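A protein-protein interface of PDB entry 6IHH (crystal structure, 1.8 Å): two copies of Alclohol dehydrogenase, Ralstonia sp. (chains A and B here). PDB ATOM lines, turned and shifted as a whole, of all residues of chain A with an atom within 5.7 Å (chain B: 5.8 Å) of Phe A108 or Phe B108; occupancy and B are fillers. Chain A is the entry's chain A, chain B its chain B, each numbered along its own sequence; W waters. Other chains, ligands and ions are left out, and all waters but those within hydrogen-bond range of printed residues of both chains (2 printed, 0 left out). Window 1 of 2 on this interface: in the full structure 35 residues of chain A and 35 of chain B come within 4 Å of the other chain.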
ATOM      1  N   HIS A 103     -17.818   1.565 -17.728  1.00  0.00           N
ATOM      2  CA  HIS A 103     -16.369   1.709 -17.793  1.00  0.00           C
ATOM      3  C   HIS A 103     -15.851   2.383 -16.518  1.00  0.00           C
ATOM      4  O   HIS A 103     -14.843   1.977 -15.952  1.00  0.00           O
ATOM      5  CB  HIS A 103     -15.964   2.508 -19.045  1.00  0.00           C
ATOM      6  CG  HIS A 103     -14.588   3.096 -18.955  1.00  0.00           C
ATOM      7  ND1 HIS A 103     -13.431   2.330 -19.178  1.00  0.00           N
ATOM      8  CD2 HIS A 103     -14.157   4.312 -18.534  1.00  0.00           C
ATOM      9  CE1 HIS A 103     -12.363   3.114 -19.053  1.00  0.00           C
ATOM     10  NE2 HIS A 103     -12.788   4.358 -18.714  1.00  0.00           N
ATOM     11  N   TYR A 104     -16.510   3.466 -16.098  1.00  0.00           N
ATOM     12  CA  TYR A 104     -16.090   4.154 -14.894  1.00  0.00           C
ATOM     13  C   TYR A 104     -16.078   3.165 -13.735  1.00  0.00           C
ATOM     14  O   TYR A 104     -15.142   3.135 -12.943  1.00  0.00           O
ATOM     15  CB  TYR A 104     -17.026   5.337 -14.621  1.00  0.00           C
ATOM     16  CG  TYR A 104     -16.906   5.927 -13.241  1.00  0.00           C
ATOM     17  CD1 TYR A 104     -15.909   6.851 -12.944  1.00  0.00           C
ATOM     18  CD2 TYR A 104     -17.741   5.509 -12.223  1.00  0.00           C
ATOM     19  CE1 TYR A 104     -15.758   7.346 -11.654  1.00  0.00           C
ATOM     20  CE2 TYR A 104     -17.550   5.930 -10.918  1.00  0.00           C
ATOM     21  CZ  TYR A 104     -16.631   6.929 -10.658  1.00  0.00           C
ATOM     22  OH  TYR A 104     -16.468   7.330  -9.365  1.00  0.00           O
ATOM     23  N   ASP A 105     -17.195   2.459 -13.525  1.00  0.00           N
ATOM     24  CA  ASP A 105     -17.311   1.558 -12.380  1.00  0.00           C
ATOM     25  C   ASP A 105     -16.312   0.404 -12.464  1.00  0.00           C
ATOM     26  O   ASP A 105     -15.745   0.000 -11.441  1.00  0.00           O
ATOM     27  CB  ASP A 105     -18.721   0.980 -12.240  1.00  0.00           C
ATOM     28  CG  ASP A 105     -19.781   1.977 -11.816  1.00  0.00           C
ATOM     29  OD1 ASP A 105     -19.455   2.950 -11.114  1.00  0.00           O
ATOM     30  OD2 ASP A 105     -20.943   1.746 -12.164  1.00  0.00           O
ATOM     31  N   ARG A 106     -16.098  -0.136 -13.661  1.00  0.00           N
ATOM     32  CA  ARG A 106     -15.138  -1.225 -13.815  1.00  0.00           C
ATOM     33  C   ARG A 106     -13.746  -0.781 -13.355  1.00  0.00           C
ATOM     34  O   ARG A 106     -12.995  -1.563 -12.766  1.00  0.00           O
ATOM     35  CB  ARG A 106     -15.069  -1.700 -15.272  1.00  0.00           C
ATOM     36  CG  ARG A 106     -16.142  -2.734 -15.607  1.00  0.00           C
ATOM     37  CD  ARG A 106     -15.962  -3.495 -16.905  1.00  0.00           C
ATOM     38  NE  ARG A 106     -15.622  -2.591 -17.995  1.00  0.00           N
ATOM     39  CZ  ARG A 106     -16.509  -2.037 -18.827  1.00  0.00           C
ATOM     40  NH1 ARG A 106     -17.790  -2.361 -18.747  1.00  0.00           N
ATOM     41  NH2 ARG A 106     -16.108  -1.206 -19.772  1.00  0.00           N
ATOM     42  N   THR A 107     -13.358   0.448 -13.720  1.00  0.00           N
ATOM     43  CA  THR A 107     -12.027   0.948 -13.385  1.00  0.00           C
ATOM     44  C   THR A 107     -11.926   1.221 -11.892  1.00  0.00           C
ATOM     45  O   THR A 107     -10.988   0.762 -11.229  1.00  0.00           O
ATOM     46  CB  THR A 107     -11.689   2.218 -14.168  1.00  0.00           C
ATOM     47  OG1 THR A 107     -11.679   1.854 -15.549  1.00  0.00           O
ATOM     48  CG2 THR A 107     -10.326   2.765 -13.804  1.00  0.00           C
ATOM     49  N   PHE A 108     -12.882   1.986 -11.364  1.00  0.00           N
ATOM     50  CA  PHE A 108     -12.795   2.373  -9.952  1.00  0.00           C
ATOM     51  C   PHE A 108     -13.025   1.195  -8.993  1.00  0.00           C
ATOM     52  O   PHE A 108     -12.499   1.187  -7.877  1.00  0.00           O
ATOM     53  CB  PHE A 108     -13.697   3.570  -9.654  1.00  0.00           C
ATOM     54  CG  PHE A 108     -13.018   4.889  -9.958  1.00  0.00           C
ATOM     55  CD1 PHE A 108     -12.841   5.320 -11.261  1.00  0.00           C
ATOM     56  CD2 PHE A 108     -12.473   5.645  -8.941  1.00  0.00           C
ATOM     57  CE1 PHE A 108     -12.258   6.553 -11.531  1.00  0.00           C
ATOM     58  CE2 PHE A 108     -11.717   6.774  -9.232  1.00  0.00           C
ATOM     59  CZ  PHE A 108     -11.609   7.224 -10.529  1.00  0.00           C
ATOM     60  N   ASP A 109     -13.842   0.214  -9.399  1.00  0.00           N
ATOM     61  CA  ASP A 109     -14.196  -0.873  -8.496  1.00  0.00           C
ATOM     62  C   ASP A 109     -12.968  -1.726  -8.170  1.00  0.00           C
ATOM     63  O   ASP A 109     -12.767  -2.070  -7.011  1.00  0.00           O
ATOM     64  CB  ASP A 109     -15.288  -1.774  -9.078  1.00  0.00           C
ATOM     65  CG  ASP A 109     -16.680  -1.198  -8.926  1.00  0.00           C
ATOM     66  OD1 ASP A 109     -16.813  -0.139  -8.300  1.00  0.00           O
ATOM     67  OD2 ASP A 109     -17.564  -1.709  -9.597  1.00  0.00           O
ATOM     68  N   VAL A 110     -12.114  -1.997  -9.161  1.00  0.00           N
ATOM     69  CA  VAL A 110     -10.938  -2.815  -8.883  1.00  0.00           C
ATOM     70  C   VAL A 110      -9.780  -1.940  -8.380  1.00  0.00           C
ATOM     71  O   VAL A 110      -9.117  -2.271  -7.398  1.00  0.00           O
ATOM     72  CB  VAL A 110     -10.545  -3.713 -10.080  1.00  0.00           C
ATOM     73  CG1 VAL A 110     -10.207  -2.915 -11.332  1.00  0.00           C
ATOM     74  CG2 VAL A 110      -9.370  -4.621  -9.739  1.00  0.00           C
ATOM     75  N   ASN A 111      -9.600  -0.755  -8.973  1.00  0.00           N
ATOM     76  CA  ASN A 111      -8.377   0.005  -8.700  1.00  0.00           C
ATOM     77  C   ASN A 111      -8.467   0.778  -7.409  1.00  0.00           C
ATOM     78  O   ASN A 111      -7.437   0.943  -6.753  1.00  0.00           O
ATOM     79  CB  ASN A 111      -7.985   0.989  -9.798  1.00  0.00           C
ATOM     80  CG  ASN A 111      -7.505   0.279 -11.044  1.00  0.00           C
ATOM     81  OD1 ASN A 111      -6.483  -0.408 -11.009  1.00  0.00           O
ATOM     82  ND2 ASN A 111      -8.308   0.301 -12.088  1.00  0.00           N
ATOM     83  N   VAL A 112      -9.680   1.221  -7.023  1.00  0.00           N
ATOM     84  CA  VAL A 112      -9.817   2.007  -5.800  1.00  0.00           C
ATOM     85  C   VAL A 112     -10.663   1.263  -4.763  1.00  0.00           C
ATOM     86  O   VAL A 112     -10.210   1.040  -3.636  1.00  0.00           O
ATOM     87  CB  VAL A 112     -10.380   3.419  -6.084  1.00  0.00           C
ATOM     88  CG1 VAL A 112     -10.365   4.282  -4.821  1.00  0.00           C
ATOM     89  CG2 VAL A 112      -9.620   4.081  -7.219  1.00  0.00           C
ATOM     90  N   ARG A 113     -11.934   0.980  -5.097  1.00  0.00           N
ATOM     91  CA  ARG A 113     -12.856   0.442  -4.106  1.00  0.00           C
ATOM     92  C   ARG A 113     -12.300  -0.873  -3.551  1.00  0.00           C
ATOM     93  O   ARG A 113     -12.243  -1.079  -2.335  1.00  0.00           O
ATOM     94  CB  ARG A 113     -14.224   0.208  -4.761  1.00  0.00           C
ATOM     95  CG  ARG A 113     -15.293  -0.288  -3.795  1.00  0.00           C
ATOM     96  CD  ARG A 113     -16.221  -1.321  -4.442  1.00  0.00           C
ATOM     97  NE  ARG A 113     -17.516  -1.463  -3.786  1.00  0.00           N
ATOM     98  CZ  ARG A 113     -18.427  -0.502  -3.798  1.00  0.00           C
ATOM     99  NH1 ARG A 113     -18.240   0.533  -4.592  1.00  0.00           N
ATOM    100  NH2 ARG A 113     -19.584  -0.665  -3.187  1.00  0.00           N
ATOM    101  N   GLY A 114     -11.931  -1.772  -4.462  1.00  0.00           N
ATOM    102  CA  GLY A 114     -11.378  -3.069  -4.083  1.00  0.00           C
ATOM    103  C   GLY A 114     -10.122  -2.964  -3.220  1.00  0.00           C
ATOM    104  O   GLY A 114      -9.891  -3.783  -2.324  1.00  0.00           O
ATOM    105  N   ILE A 116      -9.341  -0.334  -1.289  1.00  0.00           N
ATOM    106  CA  ILE A 116      -9.696   0.138   0.051  1.00  0.00           C
ATOM    107  C   ILE A 116     -10.101  -1.051   0.941  1.00  0.00           C
ATOM    108  O   ILE A 116      -9.672  -1.152   2.093  1.00  0.00           O
ATOM    109  CB  ILE A 116     -10.808   1.214  -0.054  1.00  0.00           C
ATOM    110  CG1 ILE A 116     -10.187   2.532  -0.534  1.00  0.00           C
ATOM    111  CG2 ILE A 116     -11.484   1.422   1.293  1.00  0.00           C
ATOM    112  CD1 ILE A 116     -11.208   3.594  -0.888  1.00  0.00           C
ATOM    113  N   THR A 149     -10.070   7.479 -16.571  1.00  0.00           N
ATOM    114  CA  THR A 149     -10.487   6.901 -15.296  1.00  0.00           C
ATOM    115  C   THR A 149      -9.328   6.189 -14.604  1.00  0.00           C
ATOM    116  O   THR A 149      -9.218   6.219 -13.375  1.00  0.00           O
ATOM    117  CB  THR A 149     -11.713   6.000 -15.466  1.00  0.00           C
ATOM    118  OG1 THR A 149     -11.336   4.939 -16.352  1.00  0.00           O
ATOM    119  CG2 THR A 149     -12.861   6.785 -16.083  1.00  0.00           C
ATOM    120  N   TYR A 150      -8.486   5.524 -15.392  1.00  0.00           N
ATOM    121  CA  TYR A 150      -7.420   4.727 -14.799  1.00  0.00           C
ATOM    122  C   TYR A 150      -6.428   5.646 -14.082  1.00  0.00           C
ATOM    123  O   TYR A 150      -6.087   5.427 -12.923  1.00  0.00           O
ATOM    124  CB  TYR A 150      -6.675   3.950 -15.887  1.00  0.00           C
ATOM    125  CG  TYR A 150      -5.443   3.231 -15.387  1.00  0.00           C
ATOM    126  CD1 TYR A 150      -5.532   2.006 -14.741  1.00  0.00           C
ATOM    127  CD2 TYR A 150      -4.177   3.765 -15.590  1.00  0.00           C
ATOM    128  CE1 TYR A 150      -4.401   1.341 -14.271  1.00  0.00           C
ATOM    129  CE2 TYR A 150      -3.041   3.124 -15.112  1.00  0.00           C
ATOM    130  CZ  TYR A 150      -3.147   1.898 -14.485  1.00  0.00           C
ATOM    131  OH  TYR A 150      -2.035   1.264 -14.023  1.00  0.00           O
ATOM    132  N   ALA A 152      -6.987   8.639 -12.960  1.00  0.00           N
ATOM    133  CA  ALA A 152      -7.628   9.245 -11.796  1.00  0.00           C
ATOM    134  C   ALA A 152      -7.683   8.230 -10.645  1.00  0.00           C
ATOM    135  O   ALA A 152      -7.442   8.559  -9.481  1.00  0.00           O
ATOM    136  CB  ALA A 152      -8.991   9.793 -12.177  1.00  0.00           C
ATOM    137  N   ALA A 153      -8.057   6.981 -10.962  1.00  0.00           N
ATOM    138  CA  ALA A 153      -8.066   5.938  -9.937  1.00  0.00           C
ATOM    139  C   ALA A 153      -6.671   5.779  -9.310  1.00  0.00           C
ATOM    140  O   ALA A 153      -6.533   5.608  -8.096  1.00  0.00           O
ATOM    141  CB  ALA A 153      -8.518   4.621 -10.543  1.00  0.00           C
ATOM    142  N   ALA A 156      -6.010   8.419  -6.897  1.00  0.00           N
ATOM    143  CA  ALA A 156      -6.729   8.117  -5.656  1.00  0.00           C
ATOM    144  C   ALA A 156      -5.906   7.133  -4.807  1.00  0.00           C
ATOM    145  O   ALA A 156      -5.827   7.248  -3.587  1.00  0.00           O
ATOM    146  CB  ALA A 156      -8.066   7.499  -6.018  1.00  0.00           C
ATOM    147  N   HIS B 103     -20.819   4.668   1.912  1.00  0.00           N
ATOM    148  CA  HIS B 103     -20.047   5.881   2.129  1.00  0.00           C
ATOM    149  C   HIS B 103     -19.067   6.085   0.969  1.00  0.00           C
ATOM    150  O   HIS B 103     -18.892   7.205   0.506  1.00  0.00           O
ATOM    151  CB  HIS B 103     -19.284   5.831   3.458  1.00  0.00           C
ATOM    152  CG  HIS B 103     -18.109   6.766   3.488  1.00  0.00           C
ATOM    153  ND1 HIS B 103     -18.253   8.114   3.804  1.00  0.00           N
ATOM    154  CD2 HIS B 103     -16.781   6.574   3.272  1.00  0.00           C
ATOM    155  CE1 HIS B 103     -17.066   8.705   3.757  1.00  0.00           C
ATOM    156  NE2 HIS B 103     -16.140   7.764   3.553  1.00  0.00           N
ATOM    157  N   TYR B 104     -18.435   5.001   0.489  1.00  0.00           N
ATOM    158  CA  TYR B 104     -17.523   5.157  -0.639  1.00  0.00           C
ATOM    159  C   TYR B 104     -18.311   5.662  -1.854  1.00  0.00           C
ATOM    160  O   TYR B 104     -17.845   6.523  -2.602  1.00  0.00           O
ATOM    161  CB  TYR B 104     -16.886   3.800  -0.958  1.00  0.00           C
ATOM    162  CG  TYR B 104     -16.161   3.744  -2.277  1.00  0.00           C
ATOM    163  CD1 TYR B 104     -16.851   3.507  -3.460  1.00  0.00           C
ATOM    164  CD2 TYR B 104     -14.788   3.982  -2.341  1.00  0.00           C
ATOM    165  CE1 TYR B 104     -16.197   3.475  -4.682  1.00  0.00           C
ATOM    166  CE2 TYR B 104     -14.137   4.045  -3.563  1.00  0.00           C
ATOM    167  CZ  TYR B 104     -14.840   3.763  -4.723  1.00  0.00           C
ATOM    168  OH  TYR B 104     -14.176   3.830  -5.909  1.00  0.00           O
ATOM    169  N   ASP B 105     -19.440   5.002  -2.146  1.00  0.00           N
ATOM    170  CA  ASP B 105     -20.196   5.305  -3.355  1.00  0.00           C
ATOM    171  C   ASP B 105     -20.714   6.736  -3.311  1.00  0.00           C
ATOM    172  O   ASP B 105     -20.670   7.434  -4.310  1.00  0.00           O
ATOM    173  CB  ASP B 105     -21.328   4.292  -3.608  1.00  0.00           C
ATOM    174  CG  ASP B 105     -20.840   2.899  -3.971  1.00  0.00           C
ATOM    175  OD1 ASP B 105     -19.829   2.774  -4.681  1.00  0.00           O
ATOM    176  OD2 ASP B 105     -21.522   1.961  -3.614  1.00  0.00           O
ATOM    177  N   ARG B 106     -21.226   7.189  -2.167  1.00  0.00           N
ATOM    178  CA  ARG B 106     -21.677   8.578  -2.087  1.00  0.00           C
ATOM    179  C   ARG B 106     -20.522   9.532  -2.403  1.00  0.00           C
ATOM    180  O   ARG B 106     -20.713  10.539  -3.085  1.00  0.00           O
ATOM    181  CB  ARG B 106     -22.148   8.969  -0.677  1.00  0.00           C
ATOM    182  CG  ARG B 106     -23.540   8.488  -0.290  1.00  0.00           C
ATOM    183  CD  ARG B 106     -24.023   9.051   1.045  1.00  0.00           C
ATOM    184  NE  ARG B 106     -23.219   8.611   2.183  1.00  0.00           N
ATOM    185  CZ  ARG B 106     -23.442   7.520   2.924  1.00  0.00           C
ATOM    186  NH1 ARG B 106     -24.437   6.690   2.642  1.00  0.00           N
ATOM    187  NH2 ARG B 106     -22.644   7.241   3.936  1.00  0.00           N
ATOM    188  N   THR B 107     -19.361   9.301  -1.782  1.00  0.00           N
ATOM    189  CA  THR B 107     -18.204  10.169  -1.969  1.00  0.00           C
ATOM    190  C   THR B 107     -17.788  10.218  -3.439  1.00  0.00           C
ATOM    191  O   THR B 107     -17.585  11.306  -3.987  1.00  0.00           O
ATOM    192  CB  THR B 107     -17.028   9.798  -1.055  1.00  0.00           C
ATOM    193  OG1 THR B 107     -17.483   9.999   0.290  1.00  0.00           O
ATOM    194  CG2 THR B 107     -15.815  10.668  -1.315  1.00  0.00           C
ATOM    195  N   PHE B 108     -17.568   9.046  -4.047  1.00  0.00           N
ATOM    196  CA  PHE B 108     -17.042   9.010  -5.401  1.00  0.00           C
ATOM    197  C   PHE B 108     -18.100   9.467  -6.405  1.00  0.00           C
ATOM    198  O   PHE B 108     -17.749  10.018  -7.448  1.00  0.00           O
ATOM    199  CB  PHE B 108     -16.374   7.662  -5.743  1.00  0.00           C
ATOM    200  CG  PHE B 108     -14.950   7.596  -5.259  1.00  0.00           C
ATOM    201  CD1 PHE B 108     -14.691   7.371  -3.922  1.00  0.00           C
ATOM    202  CD2 PHE B 108     -13.900   7.917  -6.101  1.00  0.00           C
ATOM    203  CE1 PHE B 108     -13.394   7.466  -3.441  1.00  0.00           C
ATOM    204  CE2 PHE B 108     -12.600   7.943  -5.629  1.00  0.00           C
ATOM    205  CZ  PHE B 108     -12.365   7.817  -4.279  1.00  0.00           C
ATOM    206  N   ASP B 109     -19.382   9.159  -6.136  1.00  0.00           N
ATOM    207  CA  ASP B 109     -20.460   9.559  -7.032  1.00  0.00           C
ATOM    208  C   ASP B 109     -20.418  11.080  -7.219  1.00  0.00           C
ATOM    209  O   ASP B 109     -20.568  11.541  -8.342  1.00  0.00           O
ATOM    210  CB  ASP B 109     -21.838   9.089  -6.523  1.00  0.00           C
ATOM    211  CG  ASP B 109     -22.136   7.645  -6.865  1.00  0.00           C
ATOM    212  OD1 ASP B 109     -21.283   7.030  -7.548  1.00  0.00           O
ATOM    213  OD2 ASP B 109     -23.147   7.114  -6.340  1.00  0.00           O
ATOM    214  N   VAL B 110     -20.432  11.842  -6.113  1.00  0.00           N
ATOM    215  CA  VAL B 110     -20.591  13.289  -6.260  1.00  0.00           C
ATOM    216  C   VAL B 110     -19.264  13.954  -6.649  1.00  0.00           C
ATOM    217  O   VAL B 110     -19.242  14.814  -7.532  1.00  0.00           O
ATOM    218  CB  VAL B 110     -21.230  14.000  -5.052  1.00  0.00           C
ATOM    219  CG1 VAL B 110     -20.408  13.852  -3.798  1.00  0.00           C
ATOM    220  CG2 VAL B 110     -21.348  15.488  -5.351  1.00  0.00           C
ATOM    221  N   ASN B 111     -18.146  13.463  -6.096  1.00  0.00           N
ATOM    222  CA  ASN B 111     -16.861  14.134  -6.309  1.00  0.00           C
ATOM    223  C   ASN B 111     -16.183  13.719  -7.617  1.00  0.00           C
ATOM    224  O   ASN B 111     -15.454  14.504  -8.218  1.00  0.00           O
ATOM    225  CB  ASN B 111     -15.903  13.919  -5.129  1.00  0.00           C
ATOM    226  CG  ASN B 111     -16.359  14.665  -3.893  1.00  0.00           C
ATOM    227  OD1 ASN B 111     -16.281  15.903  -3.854  1.00  0.00           O
ATOM    228  ND2 ASN B 111     -16.819  13.924  -2.887  1.00  0.00           N
ATOM    229  N   VAL B 112     -16.459  12.512  -8.119  1.00  0.00           N
ATOM    230  CA  VAL B 112     -15.728  12.042  -9.283  1.00  0.00           C
ATOM    231  C   VAL B 112     -16.691  11.719 -10.421  1.00  0.00           C
ATOM    232  O   VAL B 112     -16.570  12.271 -11.525  1.00  0.00           O
ATOM    233  CB  VAL B 112     -14.817  10.831  -8.985  1.00  0.00           C
ATOM    234  CG1 VAL B 112     -13.968  10.500 -10.203  1.00  0.00           C
ATOM    235  CG2 VAL B 112     -13.898  11.119  -7.806  1.00  0.00           C
ATOM    236  N   ARG B 113     -17.658  10.822 -10.157  1.00  0.00           N
ATOM    237  CA  ARG B 113     -18.520  10.356 -11.228  1.00  0.00           C
ATOM    238  C   ARG B 113     -19.237  11.555 -11.837  1.00  0.00           C
ATOM    239  O   ARG B 113     -19.254  11.732 -13.058  1.00  0.00           O
ATOM    240  CB  ARG B 113     -19.567   9.357 -10.724  1.00  0.00           C
ATOM    241  CG  ARG B 113     -20.288   8.626 -11.856  1.00  0.00           C
ATOM    242  CD  ARG B 113     -21.649   8.120 -11.398  1.00  0.00           C
ATOM    243  NE  ARG B 113     -21.405   6.960 -10.560  1.00  0.00           N
ATOM    244  CZ  ARG B 113     -21.433   5.716 -11.011  1.00  0.00           C
ATOM    245  NH1 ARG B 113     -21.136   4.700 -10.214  1.00  0.00           N
ATOM    246  NH2 ARG B 113     -21.779   5.495 -12.265  1.00  0.00           N
ATOM    247  N   GLY B 114     -19.902  12.324 -10.985  1.00  0.00           N
ATOM    248  CA  GLY B 114     -20.723  13.404 -11.509  1.00  0.00           C
ATOM    249  C   GLY B 114     -19.880  14.488 -12.181  1.00  0.00           C
ATOM    250  O   GLY B 114     -20.342  15.212 -13.065  1.00  0.00           O
ATOM    251  N   ILE B 116     -17.097  13.878 -13.816  1.00  0.00           N
ATOM    252  CA  ILE B 116     -16.744  13.369 -15.133  1.00  0.00           C
ATOM    253  C   ILE B 116     -17.902  13.610 -16.109  1.00  0.00           C
ATOM    254  O   ILE B 116     -17.676  14.088 -17.225  1.00  0.00           O
ATOM    255  CB  ILE B 116     -16.332  11.884 -15.091  1.00  0.00           C
ATOM    256  CG1 ILE B 116     -14.964  11.732 -14.401  1.00  0.00           C
ATOM    257  CG2 ILE B 116     -16.286  11.282 -16.486  1.00  0.00           C
ATOM    258  CD1 ILE B 116     -14.611  10.272 -14.139  1.00  0.00           C
ATOM    259  N   THR B 149     -11.823   8.643   1.737  1.00  0.00           N
ATOM    260  CA  THR B 149     -12.472   8.648   0.431  1.00  0.00           C
ATOM    261  C   THR B 149     -12.413  10.057  -0.166  1.00  0.00           C
ATOM    262  O   THR B 149     -12.292  10.201  -1.377  1.00  0.00           O
ATOM    263  CB  THR B 149     -13.886   8.050   0.514  1.00  0.00           C
ATOM    264  OG1 THR B 149     -14.644   8.895   1.388  1.00  0.00           O
ATOM    265  CG2 THR B 149     -13.887   6.619   1.050  1.00  0.00           C
ATOM    266  N   TYR B 150     -12.714  11.086   0.637  1.00  0.00           N
ATOM    267  CA  TYR B 150     -12.800  12.447   0.118  1.00  0.00           C
ATOM    268  C   TYR B 150     -11.452  12.855  -0.488  1.00  0.00           C
ATOM    269  O   TYR B 150     -11.365  13.376  -1.593  1.00  0.00           O
ATOM    270  CB  TYR B 150     -13.163  13.425   1.250  1.00  0.00           C
ATOM    271  CG  TYR B 150     -13.212  14.862   0.811  1.00  0.00           C
ATOM    272  CD1 TYR B 150     -14.303  15.357   0.104  1.00  0.00           C
ATOM    273  CD2 TYR B 150     -12.163  15.720   1.070  1.00  0.00           C
ATOM    274  CE1 TYR B 150     -14.315  16.655  -0.394  1.00  0.00           C
ATOM    275  CE2 TYR B 150     -12.194  17.041   0.652  1.00  0.00           C
ATOM    276  CZ  TYR B 150     -13.290  17.518  -0.037  1.00  0.00           C
ATOM    277  OH  TYR B 150     -13.280  18.808  -0.470  1.00  0.00           O
ATOM    278  N   ALA B 152      -8.977  10.965  -1.522  1.00  0.00           N
ATOM    279  CA  ALA B 152      -8.691  10.158  -2.711  1.00  0.00           C
ATOM    280  C   ALA B 152      -9.499  10.685  -3.905  1.00  0.00           C
ATOM    281  O   ALA B 152      -9.013  10.741  -5.042  1.00  0.00           O
ATOM    282  CB  ALA B 152      -8.984   8.682  -2.453  1.00  0.00           C
ATOM    283  N   ALA B 153     -10.772  10.984  -3.659  1.00  0.00           N
ATOM    284  CA  ALA B 153     -11.623  11.499  -4.727  1.00  0.00           C
ATOM    285  C   ALA B 153     -11.071  12.838  -5.226  1.00  0.00           C
ATOM    286  O   ALA B 153     -11.074  13.089  -6.429  1.00  0.00           O
ATOM    287  CB  ALA B 153     -13.063  11.647  -4.230  1.00  0.00           C
ATOM    288  N   ALA B 156      -8.271  12.313  -7.464  1.00  0.00           N
ATOM    289  CA  ALA B 156      -8.745  11.865  -8.759  1.00  0.00           C
ATOM    290  C   ALA B 156      -9.164  13.080  -9.589  1.00  0.00           C
ATOM    291  O   ALA B 156      -8.924  13.133 -10.795  1.00  0.00           O
ATOM    292  CB  ALA B 156      -9.890  10.875  -8.609  1.00  0.00           C
HETATM  293  O   HOH W   1     -15.933   4.859  -7.767  1.00  0.00           O
HETATM  294  O   HOH W   2     -18.650   6.514  -7.804  1.00  0.00           O
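Tyr A104 touches Ile B116, and with the chains exchanged Ile A116 touches Tyr B104. Asp A105 touches Arg B113, and with the chains exchanged Arg A113 touches Asp B105. Phe A108 touches its own counterpart, Phe B108. Ala A152 touches Ala B156, and with the chains exchanged Ala A156 touches Ala B152. Of the 13 pairs that touch across the chains among the printed residues, 13 have their exchanged pair printed and touching as well.
Hydrophobic or aromatic side chains of chain B that line the printed part of chain A: Tyr B104, Phe B108, Val B112, Ile B116, Ala B152 and Ala B156. Of the 18 printed residues of chain A, 8 touch a printed residue of chain B. Hydrophobic or aromatic side chains of chain A that line the printed part of chain B: Tyr A104, Phe A108, Val A112, Ile A116, Ala A152 and Ala A156. Among the printed residues, 13 pairs touch across the chains. Among the printed residues, Asp or Glu carboxylates within 4 Å of a Lys or Arg side-chain nitrogen of the other chain: Asp A105 with Arg B113 (2.6 Å) and Arg A113 with Asp B105 (2.7 Å).
N of Arg A113 sits at hydrogen-bond distance from O of Phe A108, 2.8 Å away. N of Arg B113 is in hydrogen-bond range of O of Phe B108. OD1 of Asp B109 lies within salt-bridge range of NE of Arg B113, 3.0 Å away.
Among the printed residues, pairs that only touch across the chains: Arg A113 with Tyr B104 (3.5 Å), Ala A152 with Ala B156 (3.5 Å), Ala A156 with Ala B152 (3.5 Å), Tyr A104 with Phe B108 (3.5 Å), Phe A108 with Tyr B104 (3.7 Å), Tyr A104 with Arg B113 (3.8 Å), Val A112 with Tyr B104 (3.8 Å), Tyr A104 with Ile B116 (3.8 Å), Ile A116 with Tyr B104 (3.9 Å), Tyr A104 with Val B112 (3.9 Å) and Phe A108 with Phe B108 (3.9 Å).
The side-chain carboxylate (OD1) of Asp A105 is in salt-bridge range of the guanidinium group (NH1) of Arg B113, 2.6 Å away. NH1 of Arg A113 is in salt-bridge range of OD1 of Asp B105 (2.7 Å).
Phe A108 touches just these residues of chain B: Tyr B104 and Phe B108. Phe B108 touches two residues of chain A. Of the printed residues of chain A, Arg B113 touches Tyr A104 (3.8 Å) and Asp A105 (2.6 Å). Of the printed residues of chain B, Arg A113 touches Tyr B104 (3.5 Å) and Asp B105 (2.7 Å). Of the printed residues of chain A, Ile B116 touches Tyr A104 (3.8 Å). The nearest residue of chain A that does not touch Phe B108 is Val A112 (4.1 Å). The nearest printed residue of chain A that does not touch Ile B116 is Thr A149 (4.4 Å).
Water W2 lies within hydrogen-bond range of OD1 of Asp B109 (2.7 Å) and OH of Tyr A104 (2.8 Å). Water W1 bridges the side-chain hydroxyl (OH) of Tyr B104 (2.8 Å) and the side-chain hydroxyl (OH) of Tyr A104 (3.0 Å).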
